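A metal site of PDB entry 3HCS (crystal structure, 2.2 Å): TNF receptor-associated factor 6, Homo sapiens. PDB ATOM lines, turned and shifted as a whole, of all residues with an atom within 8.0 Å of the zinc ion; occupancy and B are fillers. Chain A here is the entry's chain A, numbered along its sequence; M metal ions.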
ATOM      1  N   ASP A 112     -11.505  18.620  22.972  1.00  0.00           N
ATOM      2  CA  ASP A 112     -11.419  20.053  23.233  1.00  0.00           C
ATOM      3  C   ASP A 112     -10.466  20.369  24.378  1.00  0.00           C
ATOM      4  O   ASP A 112     -10.490  19.724  25.427  1.00  0.00           O
ATOM      5  CB  ASP A 112     -12.795  20.643  23.526  1.00  0.00           C
ATOM      6  CG  ASP A 112     -13.626  20.847  22.269  1.00  0.00           C
ATOM      7  OD1 ASP A 112     -13.080  21.341  21.251  1.00  0.00           O
ATOM      8  OD2 ASP A 112     -14.826  20.527  22.296  1.00  0.00           O
ATOM      9  N   CYS A 113      -9.617  21.364  24.156  1.00  0.00           N
ATOM     10  CA  CYS A 113      -8.669  21.783  25.162  1.00  0.00           C
ATOM     11  C   CYS A 113      -9.469  22.311  26.342  1.00  0.00           C
ATOM     12  O   CYS A 113     -10.384  23.109  26.177  1.00  0.00           O
ATOM     13  CB  CYS A 113      -7.785  22.894  24.627  1.00  0.00           C
ATOM     14  SG  CYS A 113      -6.780  23.575  25.915  1.00  0.00           S
ATOM     15  N   PRO A 114      -9.146  21.853  27.557  1.00  0.00           N
ATOM     16  CA  PRO A 114      -9.872  22.331  28.736  1.00  0.00           C
ATOM     17  C   PRO A 114      -9.634  23.801  29.071  1.00  0.00           C
ATOM     18  O   PRO A 114     -10.298  24.341  29.958  1.00  0.00           O
ATOM     19  CB  PRO A 114      -9.390  21.373  29.837  1.00  0.00           C
ATOM     20  CG  PRO A 114      -8.004  20.985  29.372  1.00  0.00           C
ATOM     21  CD  PRO A 114      -8.213  20.769  27.901  1.00  0.00           C
ATOM     22  N   GLN A 115      -8.728  24.463  28.363  1.00  0.00           N
ATOM     23  CA  GLN A 115      -8.464  25.878  28.637  1.00  0.00           C
ATOM     24  C   GLN A 115      -8.984  26.844  27.585  1.00  0.00           C
ATOM     25  O   GLN A 115      -9.550  27.879  27.918  1.00  0.00           O
ATOM     26  CB  GLN A 115      -6.981  26.123  28.867  1.00  0.00           C
ATOM     27  CG  GLN A 115      -6.527  25.823  30.283  1.00  0.00           C
ATOM     28  CD  GLN A 115      -6.545  24.348  30.600  1.00  0.00           C
ATOM     29  OE1 GLN A 115      -5.771  23.571  30.019  1.00  0.00           O
ATOM     30  NE2 GLN A 115      -7.415  23.931  31.517  1.00  0.00           N
ATOM     31  N   CYS A 116      -8.837  26.507  26.305  1.00  0.00           N
ATOM     32  CA  CYS A 116      -9.292  27.413  25.255  1.00  0.00           C
ATOM     33  C   CYS A 116     -10.427  26.799  24.441  1.00  0.00           C
ATOM     34  O   CYS A 116     -10.855  27.359  23.425  1.00  0.00           O
ATOM     35  CB  CYS A 116      -8.142  27.774  24.322  1.00  0.00           C
ATOM     36  SG  CYS A 116      -7.624  26.444  23.181  1.00  0.00           S
ATOM     37  N   GLN A 117     -10.897  25.639  24.884  1.00  0.00           N
ATOM     38  CA  GLN A 117     -11.952  24.878  24.223  1.00  0.00           C
ATOM     39  C   GLN A 117     -11.813  24.635  22.722  1.00  0.00           C
ATOM     40  O   GLN A 117     -12.769  24.256  22.053  1.00  0.00           O
ATOM     41  CB  GLN A 117     -13.348  25.426  24.539  1.00  0.00           C
ATOM     42  CG  GLN A 117     -13.504  26.929  24.563  1.00  0.00           C
ATOM     43  CD  GLN A 117     -14.946  27.333  24.862  1.00  0.00           C
ATOM     44  OE1 GLN A 117     -15.562  26.832  25.809  1.00  0.00           O
ATOM     45  NE2 GLN A 117     -15.483  28.257  24.061  1.00  0.00           N
ATOM     46  N   ARG A 118     -10.615  24.850  22.172  1.00  0.00           N
ATOM     47  CA  ARG A 118     -10.409  24.578  20.754  1.00  0.00           C
ATOM     48  C   ARG A 118     -10.181  23.066  20.614  1.00  0.00           C
ATOM     49  O   ARG A 118      -9.681  22.418  21.532  1.00  0.00           O
ATOM     50  CB  ARG A 118      -9.169  25.301  20.217  1.00  0.00           C
ATOM     51  CG  ARG A 118      -9.276  26.812  20.124  1.00  0.00           C
ATOM     52  CD  ARG A 118      -8.159  27.327  19.207  1.00  0.00           C
ATOM     53  NE  ARG A 118      -8.199  28.779  18.993  1.00  0.00           N
ATOM     54  CZ  ARG A 118      -7.642  29.677  19.813  1.00  0.00           C
ATOM     55  NH1 ARG A 118      -6.998  29.279  20.896  1.00  0.00           N
ATOM     56  NH2 ARG A 118      -7.735  30.970  19.525  1.00  0.00           N
ATOM     57  N   PRO A 119     -10.545  22.484  19.463  1.00  0.00           N
ATOM     58  CA  PRO A 119     -10.403  21.049  19.197  1.00  0.00           C
ATOM     59  C   PRO A 119      -9.026  20.614  18.676  1.00  0.00           C
ATOM     60  O   PRO A 119      -8.444  21.251  17.806  1.00  0.00           O
ATOM     61  CB  PRO A 119     -11.498  20.788  18.176  1.00  0.00           C
ATOM     62  CG  PRO A 119     -11.431  22.020  17.326  1.00  0.00           C
ATOM     63  CD  PRO A 119     -11.284  23.146  18.360  1.00  0.00           C
ATOM     64  N   PHE A 120      -8.526  19.505  19.203  1.00  0.00           N
ATOM     65  CA  PHE A 120      -7.235  18.947  18.788  1.00  0.00           C
ATOM     66  C   PHE A 120      -7.283  17.420  18.848  1.00  0.00           C
ATOM     67  O   PHE A 120      -8.040  16.841  19.626  1.00  0.00           O
ATOM     68  CB  PHE A 120      -6.102  19.450  19.701  1.00  0.00           C
ATOM     69  CG  PHE A 120      -5.786  20.903  19.545  1.00  0.00           C
ATOM     70  CD1 PHE A 120      -4.912  21.339  18.553  1.00  0.00           C
ATOM     71  CD2 PHE A 120      -6.411  21.853  20.334  1.00  0.00           C
ATOM     72  CE1 PHE A 120      -4.670  22.704  18.359  1.00  0.00           C
ATOM     73  CE2 PHE A 120      -6.186  23.209  20.150  1.00  0.00           C
ATOM     74  CZ  PHE A 120      -5.315  23.636  19.156  1.00  0.00           C
ATOM     75  N   ILE A 125      -2.808  16.617  22.167  1.00  0.00           N
ATOM     76  CA  ILE A 125      -3.352  17.316  23.305  1.00  0.00           C
ATOM     77  C   ILE A 125      -2.414  17.734  24.442  1.00  0.00           C
ATOM     78  O   ILE A 125      -2.569  18.831  24.995  1.00  0.00           O
ATOM     79  CB  ILE A 125      -4.550  16.518  23.883  1.00  0.00           C
ATOM     80  CG1 ILE A 125      -5.566  17.507  24.457  1.00  0.00           C
ATOM     81  CG2 ILE A 125      -4.068  15.510  24.891  1.00  0.00           C
ATOM     82  CD1 ILE A 125      -6.155  18.438  23.401  1.00  0.00           C
ATOM     83  N   HIS A 128      -0.210  20.610  23.182  1.00  0.00           N
ATOM     84  CA  HIS A 128      -0.994  21.830  23.109  1.00  0.00           C
ATOM     85  C   HIS A 128      -1.225  22.451  24.479  1.00  0.00           C
ATOM     86  O   HIS A 128      -0.964  23.633  24.714  1.00  0.00           O
ATOM     87  CB  HIS A 128      -2.368  21.601  22.474  1.00  0.00           C
ATOM     88  CG  HIS A 128      -3.215  22.824  22.452  1.00  0.00           C
ATOM     89  ND1 HIS A 128      -3.007  23.860  21.563  1.00  0.00           N
ATOM     90  CD2 HIS A 128      -4.186  23.250  23.299  1.00  0.00           C
ATOM     91  CE1 HIS A 128      -3.806  24.867  21.864  1.00  0.00           C
ATOM     92  NE2 HIS A 128      -4.526  24.525  22.914  1.00  0.00           N
ATOM     93  N   ILE A 129      -1.741  21.637  25.391  1.00  0.00           N
ATOM     94  CA  ILE A 129      -2.055  22.107  26.729  1.00  0.00           C
ATOM     95  C   ILE A 129      -0.902  22.654  27.538  1.00  0.00           C
ATOM     96  O   ILE A 129      -1.095  23.605  28.271  1.00  0.00           O
ATOM     97  CB  ILE A 129      -2.794  21.008  27.521  1.00  0.00           C
ATOM     98  CG1 ILE A 129      -4.212  20.825  26.957  1.00  0.00           C
ATOM     99  CG2 ILE A 129      -2.864  21.365  29.007  1.00  0.00           C
ATOM    100  CD1 ILE A 129      -4.965  19.632  27.513  1.00  0.00           C
ATOM    101  N   LEU A 130       0.293  22.067  27.403  1.00  0.00           N
ATOM    102  CA  LEU A 130       1.430  22.520  28.181  1.00  0.00           C
ATOM    103  C   LEU A 130       2.447  23.427  27.486  1.00  0.00           C
ATOM    104  O   LEU A 130       3.223  24.091  28.173  1.00  0.00           O
ATOM    105  CB  LEU A 130       2.145  21.310  28.802  1.00  0.00           C
ATOM    106  CG  LEU A 130       1.288  20.396  29.694  1.00  0.00           C
ATOM    107  CD1 LEU A 130       2.124  19.255  30.224  1.00  0.00           C
ATOM    108  CD2 LEU A 130       0.716  21.191  30.858  1.00  0.00           C
ATOM    109  N   ASP A 132       1.692  25.181  23.930  1.00  0.00           N
ATOM    110  CA  ASP A 132       1.115  26.161  22.997  1.00  0.00           C
ATOM    111  C   ASP A 132      -0.138  26.937  23.401  1.00  0.00           C
ATOM    112  O   ASP A 132      -0.356  28.043  22.936  1.00  0.00           O
ATOM    113  CB  ASP A 132       0.834  25.479  21.665  1.00  0.00           C
ATOM    114  CG  ASP A 132       1.930  24.539  21.267  1.00  0.00           C
ATOM    115  OD1 ASP A 132       3.106  24.908  21.445  1.00  0.00           O
ATOM    116  OD2 ASP A 132       1.610  23.424  20.797  1.00  0.00           O
ATOM    117  N   CYS A 133      -0.966  26.357  24.249  1.00  0.00           N
ATOM    118  CA  CYS A 133      -2.212  27.018  24.635  1.00  0.00           C
ATOM    119  C   CYS A 133      -2.057  28.421  25.221  1.00  0.00           C
ATOM    120  O   CYS A 133      -1.434  28.603  26.266  1.00  0.00           O
ATOM    121  CB  CYS A 133      -3.006  26.148  25.619  1.00  0.00           C
ATOM    122  SG  CYS A 133      -4.659  26.810  25.948  1.00  0.00           S
ATOM    123  N   PRO A 134      -2.637  29.438  24.552  1.00  0.00           N
ATOM    124  CA  PRO A 134      -2.568  30.835  25.001  1.00  0.00           C
ATOM    125  C   PRO A 134      -3.249  31.020  26.360  1.00  0.00           C
ATOM    126  O   PRO A 134      -3.016  31.988  27.063  1.00  0.00           O
ATOM    127  CB  PRO A 134      -3.293  31.601  23.895  1.00  0.00           C
ATOM    128  CG  PRO A 134      -3.043  30.744  22.671  1.00  0.00           C
ATOM    129  CD  PRO A 134      -3.261  29.355  23.215  1.00  0.00           C
ATOM    130  N   ARG A 135      -4.091  30.063  26.717  1.00  0.00           N
ATOM    131  CA  ARG A 135      -4.798  30.128  27.987  1.00  0.00           C
ATOM    132  C   ARG A 135      -4.241  29.192  29.052  1.00  0.00           C
ATOM    133  O   ARG A 135      -4.877  28.993  30.088  1.00  0.00           O
ATOM    134  CB  ARG A 135      -6.296  29.836  27.789  1.00  0.00           C
ATOM    135  CG  ARG A 135      -7.001  30.765  26.811  1.00  0.00           C
ATOM    136  CD  ARG A 135      -6.847  32.242  27.201  1.00  0.00           C
ATOM    137  NE  ARG A 135      -7.576  32.590  28.431  1.00  0.00           N
ATOM    138  CZ  ARG A 135      -7.525  33.798  29.009  1.00  0.00           C
ATOM    139  NH1 ARG A 135      -6.779  34.760  28.486  1.00  0.00           N
ATOM    140  NH2 ARG A 135      -8.211  34.028  30.122  1.00  0.00           N
ATOM    141  N   ARG A 136      -3.079  28.582  28.797  1.00  0.00           N
ATOM    142  CA  ARG A 136      -2.467  27.695  29.786  1.00  0.00           C
ATOM    143  C   ARG A 136      -2.127  28.578  30.989  1.00  0.00           C
ATOM    144  O   ARG A 136      -1.738  29.737  30.827  1.00  0.00           O
ATOM    145  CB  ARG A 136      -1.197  27.043  29.223  1.00  0.00           C
ATOM    146  CG  ARG A 136       0.087  27.805  29.499  1.00  0.00           C
ATOM    147  CD  ARG A 136       1.245  27.359  28.630  1.00  0.00           C
ATOM    148  NE  ARG A 136       1.030  27.819  27.262  1.00  0.00           N
ATOM    149  CZ  ARG A 136       1.949  28.405  26.509  1.00  0.00           C
ATOM    150  NH1 ARG A 136       3.172  28.605  26.992  1.00  0.00           N
ATOM    151  NH2 ARG A 136       1.627  28.818  25.299  1.00  0.00           N
HETATM  152 ZN    ZN M   1      -5.931  25.257  24.546  1.00  0.00          ZN
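Of the 18 residues printed, 4 come within 4 Å of the zinc ion.
The backbone NH (N) of Gln 115 sits close to the side-chain sulfur (SG) of Cys 113, at 3.3 Å.
The backbone NH of Cys 113 lies within hydrogen-bond range of the backbone carbonyl oxygen of Arg 118 (2.8 Å).
The backbone NH of Arg 135 lies close to the side-chain sulfur of Cys 133 (3.4 Å).
O of Cys 133 is in hydrogen-bond range of NE of Arg 136.
The backbone NH (N) of Arg 118 sits close to the side-chain sulfur (SG) of Cys 116, 3.5 Å away.
NE2 of His 128 binds the zinc ion.
SG of Cys 113 binds the zinc ion, 2.3 Å away.
SG of Cys 133 is bound to the zinc ion (2.4 Å).
SG of Cys 116 is bound to the zinc ion, 2.5 Å away.
The zinc ion has four donor atoms within binding distance.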
